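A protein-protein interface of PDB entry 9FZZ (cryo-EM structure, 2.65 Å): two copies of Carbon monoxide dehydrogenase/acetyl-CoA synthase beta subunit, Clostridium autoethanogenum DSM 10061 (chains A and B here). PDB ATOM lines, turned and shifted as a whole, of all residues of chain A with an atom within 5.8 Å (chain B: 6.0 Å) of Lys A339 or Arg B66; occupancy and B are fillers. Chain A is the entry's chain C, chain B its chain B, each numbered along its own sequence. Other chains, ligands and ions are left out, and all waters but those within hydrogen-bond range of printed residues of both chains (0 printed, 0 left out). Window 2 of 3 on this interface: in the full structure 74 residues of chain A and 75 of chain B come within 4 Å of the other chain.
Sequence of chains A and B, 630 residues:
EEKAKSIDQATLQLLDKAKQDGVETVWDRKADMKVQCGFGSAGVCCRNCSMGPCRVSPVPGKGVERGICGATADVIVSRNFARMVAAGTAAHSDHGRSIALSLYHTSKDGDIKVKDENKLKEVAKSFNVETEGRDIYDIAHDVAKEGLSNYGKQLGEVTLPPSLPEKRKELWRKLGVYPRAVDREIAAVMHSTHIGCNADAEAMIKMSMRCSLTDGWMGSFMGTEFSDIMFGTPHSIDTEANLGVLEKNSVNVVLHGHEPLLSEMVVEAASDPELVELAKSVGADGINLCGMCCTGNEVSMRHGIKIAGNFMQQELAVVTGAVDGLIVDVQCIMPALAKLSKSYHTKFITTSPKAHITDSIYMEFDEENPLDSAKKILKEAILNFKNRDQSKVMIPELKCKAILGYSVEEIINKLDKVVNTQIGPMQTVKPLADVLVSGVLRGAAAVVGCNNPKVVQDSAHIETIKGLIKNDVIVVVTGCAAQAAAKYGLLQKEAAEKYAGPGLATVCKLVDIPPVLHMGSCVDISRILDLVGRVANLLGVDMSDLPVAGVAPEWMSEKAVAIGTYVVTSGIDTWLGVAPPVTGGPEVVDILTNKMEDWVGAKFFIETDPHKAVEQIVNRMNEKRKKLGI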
ATOM      1  N   GLU A  24       4.704 -28.161  25.710  1.00  0.00           N
ATOM      2  CA  GLU A  24       3.314 -28.350  25.327  1.00  0.00           C
ATOM      3  C   GLU A  24       3.146 -29.651  24.560  1.00  0.00           C
ATOM      4  O   GLU A  24       4.028 -30.068  23.806  1.00  0.00           O
ATOM      5  CB  GLU A  24       2.806 -27.172  24.481  1.00  0.00           C
ATOM      6  CG  GLU A  24       3.307 -27.197  23.040  1.00  0.00           C
ATOM      7  CD  GLU A  24       2.632 -26.162  22.151  1.00  0.00           C
ATOM      8  OE1 GLU A  24       1.970 -25.249  22.681  1.00  0.00           O
ATOM      9  OE2 GLU A  24       2.767 -26.272  20.915  1.00  0.00           O
ATOM     10  N   ARG A  29      -2.225 -28.227  22.611  1.00  0.00           N
ATOM     11  CA  ARG A  29      -2.576 -27.586  21.344  1.00  0.00           C
ATOM     12  C   ARG A  29      -4.060 -27.762  21.033  1.00  0.00           C
ATOM     13  O   ARG A  29      -4.714 -26.823  20.567  1.00  0.00           O
ATOM     14  CB  ARG A  29      -1.695 -28.125  20.200  1.00  0.00           C
ATOM     15  CG  ARG A  29      -0.209 -27.716  20.343  1.00  0.00           C
ATOM     16  CD  ARG A  29       0.668 -28.040  19.104  1.00  0.00           C
ATOM     17  NE  ARG A  29       0.705 -29.464  18.773  1.00  0.00           N
ATOM     18  CZ  ARG A  29       1.431 -30.381  19.403  1.00  0.00           C
ATOM     19  NH1 ARG A  29       2.206 -30.074  20.431  1.00  0.00           N
ATOM     20  NH2 ARG A  29       1.369 -31.651  18.998  1.00  0.00           N
ATOM     21  N   MET A  33      -6.714 -24.720  20.457  1.00  0.00           N
ATOM     22  CA  MET A  33      -7.593 -24.570  19.307  1.00  0.00           C
ATOM     23  C   MET A  33      -9.015 -24.198  19.710  1.00  0.00           C
ATOM     24  O   MET A  33      -9.756 -23.663  18.879  1.00  0.00           O
ATOM     25  CB  MET A  33      -7.580 -25.868  18.488  1.00  0.00           C
ATOM     26  CG  MET A  33      -7.995 -25.682  17.033  1.00  0.00           C
ATOM     27  SD  MET A  33      -6.987 -24.450  16.152  1.00  0.00           S
ATOM     28  CE  MET A  33      -5.368 -25.219  16.069  1.00  0.00           C
ATOM     29  N   PRO A 335       4.837 -33.077  13.693  1.00  0.00           N
ATOM     30  CA  PRO A 335       5.962 -32.147  13.471  1.00  0.00           C
ATOM     31  C   PRO A 335       6.398 -31.449  14.746  1.00  0.00           C
ATOM     32  O   PRO A 335       7.579 -31.103  14.879  1.00  0.00           O
ATOM     33  CB  PRO A 335       5.429 -31.174  12.401  1.00  0.00           C
ATOM     34  CG  PRO A 335       3.926 -31.323  12.405  1.00  0.00           C
ATOM     35  CD  PRO A 335       3.672 -32.766  12.836  1.00  0.00           C
ATOM     36  N   ALA A 336       5.500 -31.295  15.721  1.00  0.00           N
ATOM     37  CA  ALA A 336       5.877 -30.655  16.974  1.00  0.00           C
ATOM     38  C   ALA A 336       7.054 -31.353  17.640  1.00  0.00           C
ATOM     39  O   ALA A 336       7.782 -30.717  18.414  1.00  0.00           O
ATOM     40  CB  ALA A 336       4.691 -30.634  17.955  1.00  0.00           C
ATOM     41  N   LEU A 337       7.276 -32.636  17.335  1.00  0.00           N
ATOM     42  CA  LEU A 337       8.435 -33.334  17.888  1.00  0.00           C
ATOM     43  C   LEU A 337       9.717 -32.538  17.706  1.00  0.00           C
ATOM     44  O   LEU A 337      10.520 -32.419  18.637  1.00  0.00           O
ATOM     45  CB  LEU A 337       8.592 -34.715  17.229  1.00  0.00           C
ATOM     46  CG  LEU A 337       7.624 -35.817  17.699  1.00  0.00           C
ATOM     47  CD1 LEU A 337       7.738 -37.066  16.810  1.00  0.00           C
ATOM     48  CD2 LEU A 337       7.833 -36.161  19.191  1.00  0.00           C
ATOM     49  N   ALA A 338       9.914 -31.946  16.524  1.00  0.00           N
ATOM     50  CA  ALA A 338      11.131 -31.168  16.314  1.00  0.00           C
ATOM     51  C   ALA A 338      11.299 -30.098  17.387  1.00  0.00           C
ATOM     52  O   ALA A 338      12.299 -30.076  18.114  1.00  0.00           O
ATOM     53  CB  ALA A 338      11.118 -30.541  14.915  1.00  0.00           C
ATOM     54  N   LYS A 339      10.266 -29.275  17.580  1.00  0.00           N
ATOM     55  CA  LYS A 339      10.322 -28.269  18.635  1.00  0.00           C
ATOM     56  C   LYS A 339      10.572 -28.915  19.992  1.00  0.00           C
ATOM     57  O   LYS A 339      11.485 -28.519  20.726  1.00  0.00           O
ATOM     58  CB  LYS A 339       9.030 -27.440  18.635  1.00  0.00           C
ATOM     59  CG  LYS A 339       9.025 -26.318  19.678  1.00  0.00           C
ATOM     60  CD  LYS A 339       7.717 -25.503  19.633  1.00  0.00           C
ATOM     61  CE  LYS A 339       7.740 -24.390  20.690  1.00  0.00           C
ATOM     62  NZ  LYS A 339       6.494 -23.551  20.656  1.00  0.00           N
ATOM     63  N   LEU A 340       9.846 -29.997  20.284  1.00  0.00           N
ATOM     64  CA  LEU A 340       9.987 -30.666  21.573  1.00  0.00           C
ATOM     65  C   LEU A 340      11.409 -31.168  21.786  1.00  0.00           C
ATOM     66  O   LEU A 340      11.954 -31.048  22.890  1.00  0.00           O
ATOM     67  CB  LEU A 340       8.960 -31.803  21.681  1.00  0.00           C
ATOM     68  CG  LEU A 340       8.920 -32.599  22.999  1.00  0.00           C
ATOM     69  CD1 LEU A 340       8.494 -31.699  24.183  1.00  0.00           C
ATOM     70  CD2 LEU A 340       8.008 -33.834  22.874  1.00  0.00           C
ATOM     71  N   SER A 341      12.068 -31.634  20.720  1.00  0.00           N
ATOM     72  CA  SER A 341      13.419 -32.184  20.834  1.00  0.00           C
ATOM     73  C   SER A 341      14.440 -31.148  21.273  1.00  0.00           C
ATOM     74  O   SER A 341      15.490 -31.515  21.805  1.00  0.00           O
ATOM     75  CB  SER A 341      13.869 -32.822  19.519  1.00  0.00           C
ATOM     76  OG  SER A 341      13.274 -34.103  19.385  1.00  0.00           O
ATOM     77  N   LYS A 342      14.129 -29.862  21.124  1.00  0.00           N
ATOM     78  CA  LYS A 342      15.041 -28.814  21.579  1.00  0.00           C
ATOM     79  C   LYS A 342      15.092 -28.744  23.098  1.00  0.00           C
ATOM     80  O   LYS A 342      16.111 -28.335  23.662  1.00  0.00           O
ATOM     81  CB  LYS A 342      14.630 -27.457  21.006  1.00  0.00           C
ATOM     82  CG  LYS A 342      14.306 -27.497  19.513  1.00  0.00           C
ATOM     83  CD  LYS A 342      15.503 -27.990  18.686  1.00  0.00           C
ATOM     84  CE  LYS A 342      15.050 -28.447  17.288  1.00  0.00           C
ATOM     85  NZ  LYS A 342      14.097 -27.455  16.675  1.00  0.00           N
ATOM     86  N   SER A 343      14.025 -29.157  23.777  1.00  0.00           N
ATOM     87  CA  SER A 343      13.978 -29.092  25.233  1.00  0.00           C
ATOM     88  C   SER A 343      14.719 -30.254  25.888  1.00  0.00           C
ATOM     89  O   SER A 343      14.825 -30.284  27.118  1.00  0.00           O
ATOM     90  CB  SER A 343      12.521 -29.070  25.734  1.00  0.00           C
ATOM     91  OG  SER A 343      11.863 -27.855  25.381  1.00  0.00           O
ATOM     92  N   CYS B  54      -8.134 -27.181  11.993  1.00  0.00           N
ATOM     93  CA  CYS B  54      -7.196 -26.296  12.675  1.00  0.00           C
ATOM     94  C   CYS B  54      -7.026 -25.021  11.866  1.00  0.00           C
ATOM     95  O   CYS B  54      -6.886 -25.064  10.637  1.00  0.00           O
ATOM     96  CB  CYS B  54      -5.810 -26.941  12.877  1.00  0.00           C
ATOM     97  SG  CYS B  54      -5.753 -28.384  13.972  1.00  0.00           S
ATOM     98  N   ARG B  55      -7.070 -23.891  12.552  1.00  0.00           N
ATOM     99  CA  ARG B  55      -6.756 -22.604  11.961  1.00  0.00           C
ATOM    100  C   ARG B  55      -5.711 -21.932  12.832  1.00  0.00           C
ATOM    101  O   ARG B  55      -5.839 -21.885  14.060  1.00  0.00           O
ATOM    102  CB  ARG B  55      -7.999 -21.729  11.778  1.00  0.00           C
ATOM    103  CG  ARG B  55      -8.933 -21.711  12.952  1.00  0.00           C
ATOM    104  CD  ARG B  55     -10.276 -21.122  12.526  1.00  0.00           C
ATOM    105  NE  ARG B  55     -11.184 -21.094  13.663  1.00  0.00           N
ATOM    106  CZ  ARG B  55     -12.486 -20.850  13.605  1.00  0.00           C
ATOM    107  NH1 ARG B  55     -13.099 -20.618  12.459  1.00  0.00           N
ATOM    108  NH2 ARG B  55     -13.194 -20.845  14.735  1.00  0.00           N
ATOM    109  N   VAL B  56      -4.652 -21.475  12.189  1.00  0.00           N
ATOM    110  CA  VAL B  56      -3.576 -20.763  12.843  1.00  0.00           C
ATOM    111  C   VAL B  56      -3.600 -19.327  12.331  1.00  0.00           C
ATOM    112  O   VAL B  56      -4.179 -19.015  11.289  1.00  0.00           O
ATOM    113  CB  VAL B  56      -2.217 -21.446  12.596  1.00  0.00           C
ATOM    114  CG1 VAL B  56      -2.226 -22.874  13.225  1.00  0.00           C
ATOM    115  CG2 VAL B  56      -1.893 -21.488  11.087  1.00  0.00           C
ATOM    116  N   VAL B  64      -3.016 -18.217  17.755  1.00  0.00           N
ATOM    117  CA  VAL B  64      -2.633 -19.625  17.697  1.00  0.00           C
ATOM    118  C   VAL B  64      -1.584 -19.818  16.616  1.00  0.00           C
ATOM    119  O   VAL B  64      -1.758 -19.380  15.471  1.00  0.00           O
ATOM    120  CB  VAL B  64      -3.868 -20.505  17.446  1.00  0.00           C
ATOM    121  CG1 VAL B  64      -3.486 -21.996  17.352  1.00  0.00           C
ATOM    122  CG2 VAL B  64      -4.903 -20.277  18.540  1.00  0.00           C
ATOM    123  N   GLU B  65      -0.482 -20.476  16.969  1.00  0.00           N
ATOM    124  CA  GLU B  65       0.643 -20.636  16.055  1.00  0.00           C
ATOM    125  C   GLU B  65       0.641 -21.974  15.334  1.00  0.00           C
ATOM    126  O   GLU B  65       1.036 -22.034  14.170  1.00  0.00           O
ATOM    127  CB  GLU B  65       1.975 -20.492  16.808  1.00  0.00           C
ATOM    128  CG  GLU B  65       2.056 -19.269  17.728  1.00  0.00           C
ATOM    129  CD  GLU B  65       2.020 -17.956  16.954  1.00  0.00           C
ATOM    130  OE1 GLU B  65       0.967 -17.635  16.370  1.00  0.00           O
ATOM    131  OE2 GLU B  65       3.049 -17.248  16.923  1.00  0.00           O
ATOM    132  N   ARG B  66       0.225 -23.056  15.987  1.00  0.00           N
ATOM    133  CA  ARG B  66       0.349 -24.378  15.398  1.00  0.00           C
ATOM    134  C   ARG B  66      -0.986 -25.106  15.438  1.00  0.00           C
ATOM    135  O   ARG B  66      -1.786 -24.923  16.357  1.00  0.00           O
ATOM    136  CB  ARG B  66       1.412 -25.233  16.123  1.00  0.00           C
ATOM    137  CG  ARG B  66       2.833 -24.667  16.023  1.00  0.00           C
ATOM    138  CD  ARG B  66       3.808 -25.428  16.944  1.00  0.00           C
ATOM    139  NE  ARG B  66       5.193 -25.027  16.713  1.00  0.00           N
ATOM    140  CZ  ARG B  66       6.070 -25.684  15.964  1.00  0.00           C
ATOM    141  NH1 ARG B  66       5.773 -26.834  15.384  1.00  0.00           N
ATOM    142  NH2 ARG B  66       7.290 -25.172  15.793  1.00  0.00           N
ATOM    143  N   GLY B  67      -1.184 -25.980  14.462  1.00  0.00           N
ATOM    144  CA  GLY B  67      -2.286 -26.909  14.503  1.00  0.00           C
ATOM    145  C   GLY B  67      -2.084 -27.908  15.628  1.00  0.00           C
ATOM    146  O   GLY B  67      -1.078 -27.903  16.345  1.00  0.00           O
ATOM    147  N   ILE B  68      -3.069 -28.795  15.783  1.00  0.00           N
ATOM    148  CA  ILE B  68      -3.060 -29.743  16.894  1.00  0.00           C
ATOM    149  C   ILE B  68      -1.871 -30.692  16.807  1.00  0.00           C
ATOM    150  O   ILE B  68      -1.230 -31.004  17.814  1.00  0.00           O
ATOM    151  CB  ILE B  68      -4.404 -30.488  16.968  1.00  0.00           C
ATOM    152  CG1 ILE B  68      -5.513 -29.466  17.303  1.00  0.00           C
ATOM    153  CG2 ILE B  68      -4.330 -31.630  18.005  1.00  0.00           C
ATOM    154  CD1 ILE B  68      -6.936 -29.994  17.159  1.00  0.00           C
ATOM    155  N   GLY B  70       0.907 -29.913  15.620  1.00  0.00           N
ATOM    156  CA  GLY B  70       2.092 -29.083  15.683  1.00  0.00           C
ATOM    157  C   GLY B  70       2.509 -28.421  14.379  1.00  0.00           C
ATOM    158  O   GLY B  70       3.548 -27.758  14.352  1.00  0.00           O
ATOM    159  N   ALA B  71       1.728 -28.557  13.311  1.00  0.00           N
ATOM    160  CA  ALA B  71       2.078 -27.966  12.023  1.00  0.00           C
ATOM    161  C   ALA B  71       1.992 -26.437  12.054  1.00  0.00           C
ATOM    162  O   ALA B  71       1.009 -25.869  12.534  1.00  0.00           O
ATOM    163  CB  ALA B  71       1.153 -28.531  10.940  1.00  0.00           C
ATOM    164  N   THR B  72       3.023 -25.767  11.523  1.00  0.00           N
ATOM    165  CA  THR B  72       3.067 -24.312  11.490  1.00  0.00           C
ATOM    166  C   THR B  72       2.211 -23.753  10.355  1.00  0.00           C
ATOM    167  O   THR B  72       1.703 -24.476   9.495  1.00  0.00           O
ATOM    168  CB  THR B  72       4.500 -23.795  11.322  1.00  0.00           C
ATOM    169  OG1 THR B  72       5.066 -24.307  10.104  1.00  0.00           O
ATOM    170  CG2 THR B  72       5.366 -24.192  12.514  1.00  0.00           C
ATOM    171  N   ALA B  73       2.090 -22.426  10.343  1.00  0.00           N
ATOM    172  CA  ALA B  73       1.367 -21.781   9.255  1.00  0.00           C
ATOM    173  C   ALA B  73       2.038 -22.076   7.922  1.00  0.00           C
ATOM    174  O   ALA B  73       1.364 -22.428   6.954  1.00  0.00           O
ATOM    175  CB  ALA B  73       1.257 -20.271   9.508  1.00  0.00           C
ATOM    176  N   ILE B  76       1.050 -25.600   6.840  1.00  0.00           N
ATOM    177  CA  ILE B  76      -0.349 -25.682   6.404  1.00  0.00           C
ATOM    178  C   ILE B  76      -0.512 -25.043   5.034  1.00  0.00           C
ATOM    179  O   ILE B  76      -1.164 -25.602   4.137  1.00  0.00           O
ATOM    180  CB  ILE B  76      -1.265 -25.046   7.474  1.00  0.00           C
ATOM    181  CG1 ILE B  76      -1.145 -25.859   8.787  1.00  0.00           C
ATOM    182  CG2 ILE B  76      -2.743 -24.951   6.988  1.00  0.00           C
ATOM    183  CD1 ILE B  76      -1.775 -25.226  10.015  1.00  0.00           C
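Of chain B, only Arg B66 comes within 4 Å of Lys A339. Arg B66 touches just these residues of chain A: Met A33 (3.6 Å) and Lys A339 (3.9 Å). Of the printed residues of chain A, Ala B71 touches Pro A335. Printed residues of chain A within 4 Å of Ile B68: Arg A29. Of the printed residues of chain B, Arg A29 touches Gly B67, Ile B68 and Gly B70. Of the printed residues of chain A, Gly B67 touches Arg A29 and Met A33. Of the printed residues of chain A, Cys B54 touches Met A33. The nearest printed residue of chain A that does not touch Arg B66 is Ala A336 (4.1 Å).
Among the printed residues, pairs that only touch across the chains: Met A33 with Arg B66 (3.6 Å), Pro A335 with Ala B71 (3.6 Å), Met A33 with Cys B54 (3.7 Å), Ala A336 with Gly B70 (3.8 Å), Pro A335 with Gly B70 (3.8 Å), Met A33 with Gly B67 (3.8 Å), Lys A339 with Arg B66 (3.9 Å) and Met A33 with Val B64 (3.9 Å).
No position is printed for both chains. Of the 12 pairs that touch across the chains among the printed residues, none has its exchanged pair printed and touching as well.
The guanidinium group (NE) of Arg A29 lies close to the backbone NH (N) of Gly B70 (3.2 Å). The backbone NH of Arg B55 lies within hydrogen-bond range of the side-chain sulfur of Met A33, 3.6 Å away. The guanidinium group (NE) of Arg A29 is in hydrogen-bond range of the backbone carbonyl oxygen (O) of Ile B68, 2.7 Å away. The backbone carbonyl oxygen (O) of Gly B67 lies close to the guanidinium group (NE) of Arg A29 (3.4 Å).
OE2 of Glu A24 lies within salt-bridge range of NH1 of Arg A29, at 3.9 Å. SG of Cys B54 sits close to N of Ile B68 (3.3 Å). The guanidinium group of Arg B66 sits at hydrogen-bond distance from the backbone carbonyl oxygen of Gly B70 (2.6 Å).
Of the 12 printed residues of chain A, 5 touch a printed residue of chain B. Hydrophobic or aromatic side chains of chain A that line the printed part of chain B: Met A33, Pro A335 and Ala A336. Hydrophobic or aromatic side chains of chain B within 4 Å of the printed part of chain A: Val B64. Along chain B the printed residues that touch a printed residue of chain A span positions 54 to 71. Among the printed residues, no Asp or Glu carboxylate lies within 4 Å of a Lys or Arg side-chain nitrogen of the other chain.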
